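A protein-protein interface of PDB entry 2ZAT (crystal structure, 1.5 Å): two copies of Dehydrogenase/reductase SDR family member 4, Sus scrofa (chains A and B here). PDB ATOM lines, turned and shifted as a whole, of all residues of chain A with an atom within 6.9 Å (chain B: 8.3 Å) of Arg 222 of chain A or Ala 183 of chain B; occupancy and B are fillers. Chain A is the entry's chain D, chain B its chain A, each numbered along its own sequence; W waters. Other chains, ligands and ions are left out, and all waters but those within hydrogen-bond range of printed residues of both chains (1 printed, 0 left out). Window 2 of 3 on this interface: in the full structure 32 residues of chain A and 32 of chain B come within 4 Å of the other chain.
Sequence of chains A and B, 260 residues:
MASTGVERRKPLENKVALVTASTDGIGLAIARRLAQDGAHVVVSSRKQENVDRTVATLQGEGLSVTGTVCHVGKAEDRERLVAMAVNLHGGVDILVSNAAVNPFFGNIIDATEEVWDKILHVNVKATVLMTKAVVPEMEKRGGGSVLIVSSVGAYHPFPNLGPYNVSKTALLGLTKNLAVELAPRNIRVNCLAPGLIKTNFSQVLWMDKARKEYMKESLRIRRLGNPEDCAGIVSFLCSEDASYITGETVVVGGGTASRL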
ATOM      1  N   GLU A 213     -23.815 -34.796   6.417  1.00  0.00           N
ATOM      2  CA  GLU A 213     -24.406 -35.171   7.700  1.00  0.00           C
ATOM      3  C   GLU A 213     -23.322 -35.594   8.693  1.00  0.00           C
ATOM      4  O   GLU A 213     -23.421 -35.296   9.882  1.00  0.00           O
ATOM      5  CB  GLU A 213     -25.465 -36.279   7.519  1.00  0.00           C
ATOM      6  CG  GLU A 213     -26.878 -35.920   7.984  1.00  0.00           C
ATOM      7  CD  GLU A 213     -27.257 -34.455   7.776  1.00  0.00           C
ATOM      8  OE1 GLU A 213     -27.183 -33.964   6.627  1.00  0.00           O
ATOM      9  OE2 GLU A 213     -27.635 -33.785   8.768  1.00  0.00           O
ATOM     10  N   LYS A 216     -21.687 -32.293   9.866  1.00  0.00           N
ATOM     11  CA  LYS A 216     -22.532 -31.537  10.796  1.00  0.00           C
ATOM     12  C   LYS A 216     -22.529 -32.161  12.198  1.00  0.00           C
ATOM     13  O   LYS A 216     -22.508 -31.444  13.192  1.00  0.00           O
ATOM     14  CB  LYS A 216     -23.953 -31.372  10.254  1.00  0.00           C
ATOM     15  CG  LYS A 216     -24.040 -30.331   9.140  1.00  0.00           C
ATOM     16  CD  LYS A 216     -25.317 -30.438   8.340  1.00  0.00           C
ATOM     17  CE  LYS A 216     -26.533 -30.072   9.140  1.00  0.00           C
ATOM     18  NZ  LYS A 216     -27.695 -29.882   8.241  1.00  0.00           N
ATOM     19  N   ARG A 220     -20.601 -30.511  15.231  1.00  0.00           N
ATOM     20  CA  ARG A 220     -21.657 -30.072  16.159  1.00  0.00           C
ATOM     21  C   ARG A 220     -22.333 -28.748  15.749  1.00  0.00           C
ATOM     22  O   ARG A 220     -22.492 -27.825  16.551  1.00  0.00           O
ATOM     23  CB  ARG A 220     -21.111 -29.979  17.591  1.00  0.00           C
ATOM     24  CG  ARG A 220     -22.153 -30.142  18.672  1.00  0.00           C
ATOM     25  CD  ARG A 220     -21.770 -31.142  19.780  1.00  0.00           C
ATOM     26  NE  ARG A 220     -20.601 -30.705  20.549  1.00  0.00           N
ATOM     27  CZ  ARG A 220     -19.754 -31.509  21.208  1.00  0.00           C
ATOM     28  NH1 ARG A 220     -19.917 -32.830  21.224  1.00  0.00           N
ATOM     29  NH2 ARG A 220     -18.733 -30.978  21.875  1.00  0.00           N
ATOM     30  N   ILE A 221     -22.749 -28.687  14.492  1.00  0.00           N
ATOM     31  CA  ILE A 221     -23.412 -27.524  13.915  1.00  0.00           C
ATOM     32  C   ILE A 221     -24.804 -27.859  13.362  1.00  0.00           C
ATOM     33  O   ILE A 221     -25.042 -28.985  12.923  1.00  0.00           O
ATOM     34  CB  ILE A 221     -22.545 -26.927  12.789  1.00  0.00           C
ATOM     35  CG1 ILE A 221     -22.198 -27.957  11.698  1.00  0.00           C
ATOM     36  CG2 ILE A 221     -21.258 -26.309  13.372  1.00  0.00           C
ATOM     37  CD1 ILE A 221     -21.434 -27.371  10.524  1.00  0.00           C
ATOM     38  N   ARG A 222     -25.698 -26.875  13.364  1.00  0.00           N
ATOM     39  CA  ARG A 222     -27.077 -27.049  12.841  1.00  0.00           C
ATOM     40  C   ARG A 222     -27.216 -26.849  11.341  1.00  0.00           C
ATOM     41  O   ARG A 222     -28.138 -27.376  10.712  1.00  0.00           O
ATOM     42  CB  ARG A 222     -28.033 -26.078  13.512  1.00  0.00           C
ATOM     43  CG  ARG A 222     -28.084 -26.214  15.001  1.00  0.00           C
ATOM     44  CD  ARG A 222     -28.999 -25.209  15.641  1.00  0.00           C
ATOM     45  NE  ARG A 222     -30.359 -25.264  15.101  1.00  0.00           N
ATOM     46  CZ  ARG A 222     -31.143 -24.211  14.849  1.00  0.00           C
ATOM     47  NH1 ARG A 222     -30.726 -22.965  15.055  1.00  0.00           N
ATOM     48  NH2 ARG A 222     -32.361 -24.411  14.360  1.00  0.00           N
ATOM     49  N   ARG A 223     -26.333 -26.041  10.763  1.00  0.00           N
ATOM     50  CA  ARG A 223     -26.318 -25.792   9.336  1.00  0.00           C
ATOM     51  C   ARG A 223     -24.905 -25.460   8.939  1.00  0.00           C
ATOM     52  O   ARG A 223     -24.100 -25.083   9.790  1.00  0.00           O
ATOM     53  CB  ARG A 223     -27.248 -24.633   8.945  1.00  0.00           C
ATOM     54  CG  ARG A 223     -26.812 -23.237   9.449  1.00  0.00           C
ATOM     55  CD  ARG A 223     -27.714 -22.141   8.960  1.00  0.00           C
ATOM     56  NE  ARG A 223     -27.406 -20.794   9.445  1.00  0.00           N
ATOM     57  CZ  ARG A 223     -26.575 -19.937   8.834  1.00  0.00           C
ATOM     58  NH1 ARG A 223     -25.914 -20.288   7.741  1.00  0.00           N
ATOM     59  NH2 ARG A 223     -26.412 -18.718   9.330  1.00  0.00           N
ATOM     60  N   LEU A 224     -24.630 -25.590   7.655  1.00  0.00           N
ATOM     61  CA  LEU A 224     -23.415 -25.060   7.084  1.00  0.00           C
ATOM     62  C   LEU A 224     -23.551 -23.549   6.948  1.00  0.00           C
ATOM     63  O   LEU A 224     -24.626 -22.980   6.768  1.00  0.00           O
ATOM     64  CB  LEU A 224     -23.151 -25.666   5.700  1.00  0.00           C
ATOM     65  CG  LEU A 224     -23.247 -27.189   5.632  1.00  0.00           C
ATOM     66  CD1 LEU A 224     -22.988 -27.645   4.197  1.00  0.00           C
ATOM     67  CD2 LEU A 224     -22.306 -27.805   6.601  1.00  0.00           C
ATOM     68  N   GLY A 254     -20.765 -21.120  13.578  1.00  0.00           N
ATOM     69  CA  GLY A 254     -22.059 -21.716  13.879  1.00  0.00           C
ATOM     70  C   GLY A 254     -22.064 -22.576  15.124  1.00  0.00           C
ATOM     71  O   GLY A 254     -22.986 -23.399  15.275  1.00  0.00           O
ATOM     72  N   GLY A 255     -21.087 -22.369  16.006  1.00  0.00           N
ATOM     73  CA  GLY A 255     -20.960 -23.065  17.266  1.00  0.00           C
ATOM     74  C   GLY A 255     -20.008 -24.245  17.212  1.00  0.00           C
ATOM     75  O   GLY A 255     -19.837 -24.945  18.228  1.00  0.00           O
ATOM     76  N   GLY B 142     -38.974 -17.296  18.373  1.00  0.00           N
ATOM     77  CA  GLY B 142     -38.306 -18.002  17.294  1.00  0.00           C
ATOM     78  C   GLY B 142     -36.790 -17.956  17.389  1.00  0.00           C
ATOM     79  O   GLY B 142     -36.077 -18.403  16.495  1.00  0.00           O
ATOM     80  N   GLY B 143     -36.305 -17.424  18.501  1.00  0.00           N
ATOM     81  CA  GLY B 143     -34.863 -17.332  18.727  1.00  0.00           C
ATOM     82  C   GLY B 143     -34.485 -16.081  19.478  1.00  0.00           C
ATOM     83  O   GLY B 143     -35.324 -15.300  19.879  1.00  0.00           O
ATOM     84  N   LYS B 176     -19.586 -20.895  26.392  1.00  0.00           N
ATOM     85  CA  LYS B 176     -19.488 -22.062  25.540  1.00  0.00           C
ATOM     86  C   LYS B 176     -20.558 -23.102  25.784  1.00  0.00           C
ATOM     87  O   LYS B 176     -21.112 -23.667  24.845  1.00  0.00           O
ATOM     88  CB  LYS B 176     -18.122 -22.731  25.715  1.00  0.00           C
ATOM     89  CG  LYS B 176     -16.933 -21.910  25.293  1.00  0.00           C
ATOM     90  CD  LYS B 176     -16.865 -21.784  23.809  1.00  0.00           C
ATOM     91  CE  LYS B 176     -15.508 -21.225  23.400  1.00  0.00           C
ATOM     92  NZ  LYS B 176     -15.457 -21.031  21.925  1.00  0.00           N
ATOM     93  N   ASN B 177     -20.814 -23.392  27.049  1.00  0.00           N
ATOM     94  CA  ASN B 177     -21.819 -24.393  27.402  1.00  0.00           C
ATOM     95  C   ASN B 177     -23.217 -23.924  27.009  1.00  0.00           C
ATOM     96  O   ASN B 177     -23.990 -24.694  26.492  1.00  0.00           O
ATOM     97  CB  ASN B 177     -21.760 -24.732  28.885  1.00  0.00           C
ATOM     98  CG  ASN B 177     -20.613 -25.643  29.221  1.00  0.00           C
ATOM     99  OD1 ASN B 177     -20.781 -26.867  29.200  1.00  0.00           O
ATOM    100  ND2 ASN B 177     -19.430 -25.067  29.531  1.00  0.00           N
ATOM    101  N   LEU B 178     -23.527 -22.667  27.266  1.00  0.00           N
ATOM    102  CA  LEU B 178     -24.839 -22.147  26.879  1.00  0.00           C
ATOM    103  C   LEU B 178     -24.999 -22.132  25.368  1.00  0.00           C
ATOM    104  O   LEU B 178     -26.047 -22.455  24.857  1.00  0.00           O
ATOM    105  CB  LEU B 178     -25.070 -20.733  27.429  1.00  0.00           C
ATOM    106  CG  LEU B 178     -25.330 -20.587  28.920  1.00  0.00           C
ATOM    107  CD1 LEU B 178     -25.275 -19.122  29.307  1.00  0.00           C
ATOM    108  CD2 LEU B 178     -26.681 -21.165  29.287  1.00  0.00           C
ATOM    109  N   ALA B 179     -23.962 -21.794  24.616  1.00  0.00           N
ATOM    110  CA  ALA B 179     -24.073 -21.722  23.165  1.00  0.00           C
ATOM    111  C   ALA B 179     -24.410 -23.083  22.569  1.00  0.00           C
ATOM    112  O   ALA B 179     -25.286 -23.181  21.699  1.00  0.00           O
ATOM    113  CB  ALA B 179     -22.772 -21.124  22.560  1.00  0.00           C
ATOM    114  N   VAL B 180     -23.740 -24.118  23.064  1.00  0.00           N
ATOM    115  CA  VAL B 180     -23.998 -25.492  22.598  1.00  0.00           C
ATOM    116  C   VAL B 180     -25.435 -25.893  22.888  1.00  0.00           C
ATOM    117  O   VAL B 180     -26.151 -26.424  22.037  1.00  0.00           O
ATOM    118  CB  VAL B 180     -23.030 -26.477  23.344  1.00  0.00           C
ATOM    119  CG1 VAL B 180     -23.508 -27.942  23.224  1.00  0.00           C
ATOM    120  CG2 VAL B 180     -21.606 -26.259  22.874  1.00  0.00           C
ATOM    121  N   GLU B 181     -25.868 -25.599  24.092  1.00  0.00           N
ATOM    122  CA  GLU B 181     -27.133 -26.141  24.580  1.00  0.00           C
ATOM    123  C   GLU B 181     -28.359 -25.385  24.134  1.00  0.00           C
ATOM    124  O   GLU B 181     -29.466 -25.959  24.077  1.00  0.00           O
ATOM    125  CB  GLU B 181     -27.084 -26.232  26.059  1.00  0.00           C
ATOM    126  CG  GLU B 181     -26.044 -27.252  26.423  1.00  0.00           C
ATOM    127  CD  GLU B 181     -25.998 -27.514  27.871  1.00  0.00           C
ATOM    128  OE1 GLU B 181     -26.939 -27.071  28.559  1.00  0.00           O
ATOM    129  OE2 GLU B 181     -25.021 -28.160  28.295  1.00  0.00           O
ATOM    130  N   LEU B 182     -28.180 -24.121  23.780  1.00  0.00           N
ATOM    131  CA  LEU B 182     -29.292 -23.300  23.318  1.00  0.00           C
ATOM    132  C   LEU B 182     -29.390 -23.155  21.805  1.00  0.00           C
ATOM    133  O   LEU B 182     -30.396 -22.636  21.287  1.00  0.00           O
ATOM    134  CB  LEU B 182     -29.234 -21.920  23.962  1.00  0.00           C
ATOM    135  CG  LEU B 182     -29.272 -21.888  25.479  1.00  0.00           C
ATOM    136  CD1 LEU B 182     -29.246 -20.467  26.001  1.00  0.00           C
ATOM    137  CD2 LEU B 182     -30.521 -22.626  26.024  1.00  0.00           C
ATOM    138  N   ALA B 183     -28.394 -23.657  21.072  1.00  0.00           N
ATOM    139  CA  ALA B 183     -28.406 -23.644  19.618  1.00  0.00           C
ATOM    140  C   ALA B 183     -29.665 -24.303  19.027  1.00  0.00           C
ATOM    141  O   ALA B 183     -30.227 -23.741  18.091  1.00  0.00           O
ATOM    142  CB  ALA B 183     -27.181 -24.323  19.076  1.00  0.00           C
ATOM    143  N   PRO B 184     -30.117 -25.438  19.574  1.00  0.00           N
ATOM    144  CA  PRO B 184     -31.350 -26.078  19.053  1.00  0.00           C
ATOM    145  C   PRO B 184     -32.611 -25.220  19.114  1.00  0.00           C
ATOM    146  O   PRO B 184     -33.532 -25.417  18.309  1.00  0.00           O
ATOM    147  CB  PRO B 184     -31.495 -27.325  19.938  1.00  0.00           C
ATOM    148  CG  PRO B 184     -30.160 -27.603  20.402  1.00  0.00           C
ATOM    149  CD  PRO B 184     -29.540 -26.241  20.664  1.00  0.00           C
ATOM    150  N   ARG B 185     -32.617 -24.251  20.021  1.00  0.00           N
ATOM    151  CA  ARG B 185     -33.685 -23.263  20.188  1.00  0.00           C
ATOM    152  C   ARG B 185     -33.442 -21.960  19.414  1.00  0.00           C
ATOM    153  O   ARG B 185     -34.191 -20.998  19.577  1.00  0.00           O
ATOM    154  CB  ARG B 185     -33.828 -22.957  21.676  1.00  0.00           C
ATOM    155  CG  ARG B 185     -34.205 -24.169  22.538  1.00  0.00           C
ATOM    156  CD  ARG B 185     -33.395 -24.333  23.821  1.00  0.00           C
ATOM    157  NE  ARG B 185     -34.153 -23.952  25.013  1.00  0.00           N
ATOM    158  CZ  ARG B 185     -34.402 -24.741  26.068  1.00  0.00           C
ATOM    159  NH1 ARG B 185     -35.135 -24.270  27.076  1.00  0.00           N
ATOM    160  NH2 ARG B 185     -33.928 -25.981  26.142  1.00  0.00           N
ATOM    161  N   ASN B 186     -32.408 -21.932  18.565  1.00  0.00           N
ATOM    162  CA  ASN B 186     -32.061 -20.771  17.761  1.00  0.00           C
ATOM    163  C   ASN B 186     -31.705 -19.560  18.631  1.00  0.00           C
ATOM    164  O   ASN B 186     -31.986 -18.412  18.267  1.00  0.00           O
ATOM    165  CB  ASN B 186     -33.178 -20.435  16.771  1.00  0.00           C
ATOM    166  CG  ASN B 186     -32.712 -19.550  15.633  1.00  0.00           C
ATOM    167  OD1 ASN B 186     -31.572 -19.649  15.170  1.00  0.00           O
ATOM    168  ND2 ASN B 186     -33.589 -18.651  15.179  1.00  0.00           N
ATOM    169  N   ILE B 187     -31.042 -19.825  19.746  1.00  0.00           N
ATOM    170  CA  ILE B 187     -30.570 -18.772  20.633  1.00  0.00           C
ATOM    171  C   ILE B 187     -29.051 -18.823  20.586  1.00  0.00           C
ATOM    172  O   ILE B 187     -28.463 -19.851  20.889  1.00  0.00           O
ATOM    173  CB  ILE B 187     -31.084 -18.961  22.060  1.00  0.00           C
ATOM    174  CG1 ILE B 187     -32.610 -18.791  22.070  1.00  0.00           C
ATOM    175  CG2 ILE B 187     -30.437 -17.955  22.989  1.00  0.00           C
ATOM    176  CD1 ILE B 187     -33.276 -19.275  23.332  1.00  0.00           C
ATOM    177  N   ARG B 188     -28.451 -17.698  20.216  1.00  0.00           N
ATOM    178  CA  ARG B 188     -27.001 -17.546  20.156  1.00  0.00           C
ATOM    179  C   ARG B 188     -26.508 -16.968  21.446  1.00  0.00           C
ATOM    180  O   ARG B 188     -27.176 -16.166  22.059  1.00  0.00           O
ATOM    181  CB  ARG B 188     -26.607 -16.655  18.986  1.00  0.00           C
ATOM    182  CG  ARG B 188     -26.932 -17.276  17.621  1.00  0.00           C
ATOM    183  CD  ARG B 188     -26.484 -16.475  16.405  1.00  0.00           C
ATOM    184  NE  ARG B 188     -27.148 -15.180  16.425  1.00  0.00           N
ATOM    185  CZ  ARG B 188     -26.619 -14.041  16.833  1.00  0.00           C
ATOM    186  NH1 ARG B 188     -25.352 -13.964  17.232  1.00  0.00           N
ATOM    187  NH2 ARG B 188     -27.383 -12.949  16.844  1.00  0.00           N
ATOM    188  N   VAL B 189     -25.317 -17.360  21.855  1.00  0.00           N
ATOM    189  CA  VAL B 189     -24.724 -16.882  23.099  1.00  0.00           C
ATOM    190  C   VAL B 189     -23.267 -16.541  22.834  1.00  0.00           C
ATOM    191  O   VAL B 189     -22.482 -17.426  22.408  1.00  0.00           O
ATOM    192  CB  VAL B 189     -24.785 -17.940  24.222  1.00  0.00           C
ATOM    193  CG1 VAL B 189     -24.305 -17.358  25.524  1.00  0.00           C
ATOM    194  CG2 VAL B 189     -26.211 -18.502  24.340  1.00  0.00           C
ATOM    195  N   SER B 243     -25.808 -14.227  12.556  1.00  0.00           N
ATOM    196  CA  SER B 243     -26.512 -15.482  12.793  1.00  0.00           C
ATOM    197  C   SER B 243     -25.667 -16.743  12.787  1.00  0.00           C
ATOM    198  O   SER B 243     -26.134 -17.766  13.284  1.00  0.00           O
ATOM    199  CB  SER B 243     -27.654 -15.637  11.781  1.00  0.00           C
ATOM    200  OG  SER B 243     -27.216 -15.913  10.488  1.00  0.00           O
ATOM    201  N   TYR B 244     -24.454 -16.708  12.253  1.00  0.00           N
ATOM    202  CA  TYR B 244     -23.572 -17.881  12.271  1.00  0.00           C
ATOM    203  C   TYR B 244     -22.460 -17.703  13.310  1.00  0.00           C
ATOM    204  O   TYR B 244     -21.456 -18.390  13.279  1.00  0.00           O
ATOM    205  CB  TYR B 244     -22.999 -18.201  10.871  1.00  0.00           C
ATOM    206  CG  TYR B 244     -22.675 -19.651  10.635  1.00  0.00           C
ATOM    207  CD1 TYR B 244     -23.659 -20.622  10.755  1.00  0.00           C
ATOM    208  CD2 TYR B 244     -21.399 -20.066  10.308  1.00  0.00           C
ATOM    209  CE1 TYR B 244     -23.365 -21.947  10.525  1.00  0.00           C
ATOM    210  CE2 TYR B 244     -21.105 -21.397  10.087  1.00  0.00           C
ATOM    211  CZ  TYR B 244     -22.099 -22.336  10.227  1.00  0.00           C
ATOM    212  OH  TYR B 244     -21.783 -23.689  10.007  1.00  0.00           O
ATOM    213  N   THR B 246     -21.784 -17.901  17.227  1.00  0.00           N
ATOM    214  CA  THR B 246     -22.207 -18.282  18.564  1.00  0.00           C
ATOM    215  C   THR B 246     -21.069 -18.964  19.270  1.00  0.00           C
ATOM    216  O   THR B 246     -20.223 -19.571  18.632  1.00  0.00           O
ATOM    217  CB  THR B 246     -23.520 -19.109  18.533  1.00  0.00           C
ATOM    218  OG1 THR B 246     -24.068 -19.223  19.861  1.00  0.00           O
ATOM    219  CG2 THR B 246     -23.271 -20.539  18.049  1.00  0.00           C
HETATM  220  O   HOH W   1     -28.205 -19.267  11.931  1.00  0.00           O
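O of Gly 142 of chain B sits at hydrogen-bond distance from ND2 of Asn 186 of chain B (2.8 Å).
The backbone NH (N) of Val 189 of chain B is in hydrogen-bond range of the side-chain hydroxyl (OG1) of Thr 246 of chain B, 3.0 Å away.
The backbone carbonyl oxygen (O) of Lys 216 of chain A is in hydrogen-bond range of the backbone NH (N) of Ile 221 of chain A (3.1 Å).
Of chain A, only Arg 222 (3.1 Å) comes within 4 Å of Ala 183 of chain B.
Of the printed residues of chain B, Gly 254 of chain A touches Tyr 244 (2.8 Å) and Thr 246 (3.8 Å).
Of the printed residues of chain A, Tyr 244 of chain B touches Ile 221, Arg 223, Leu 224 and Gly 254.
Printed residues of chain B within 4 Å of Gly 255 of chain A: Thr 246 (3.5 Å).
Printed residues of chain B within 4 Å of Leu 224 of chain A: Tyr 244.
Leu 182 of chain B touches none of the printed residues of chain A.
Glu 213 of chain A touches none of the printed residues of chain B.
The nearest residue of chain B that does not touch Arg 222 of chain A is Pro 184 of chain B (4.1 Å).
The nearest printed residue of chain B that does not touch Ile 221 of chain A is Ala 183 of chain B (7.1 Å).
No position is printed for both chains.
Of the 9 pairs that touch across the chains among the printed residues, none has its exchanged pair printed and touching as well.
Water W1 bridges O of Ser 243 of chain B (2.9 Å) and NE of Arg 223 of chain A (3.0 Å).
Of the 9 printed residues of chain A, 6 touch a printed residue of chain B.
Hydrophobic or aromatic side chains of chain A that line the printed part of chain B: Ile 221.
Along chain A the printed residues that touch a printed residue of chain B span positions 221 to 255.
Of the 19 printed residues of chain B, 5 touch a printed residue of chain A.
Printed residues of chain B that touch a printed residue of chain A: Ala 183, Asn 186, Ser 243, Tyr 244 and Thr 246.
Among the printed residues, 9 pairs touch across the chains.
Among the printed residues, pairs that only touch across the chains: Ile 221 of chain A with Tyr 244 of chain B (3.7 Å), Leu 224 of chain A with Tyr 244 of chain B (3.5 Å), Gly 254 of chain A with Thr 246 of chain B (3.8 Å) and Gly 255 of chain A with Thr 246 of chain B (3.5 Å).
The backbone carbonyl oxygen (O) of Ala 183 of chain B sits close to the guanidinium group (NH1) of Arg 222 of chain A (3.2 Å).
The guanidinium group (NH1) of Arg 222 of chain A lies within hydrogen-bond range of the side-chain amide oxygen (OD1) of Asn 186 of chain B, at 3.4 Å.
NH2 of Arg 223 of chain A is in hydrogen-bond range of OG of Ser 243 of chain B.
OH of Tyr 244 of chain B is in hydrogen-bond range of O of Arg 223 of chain A, 2.7 Å away.
O of Tyr 244 of chain B lies within hydrogen-bond range of N of Gly 254 of chain A (2.8 Å).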
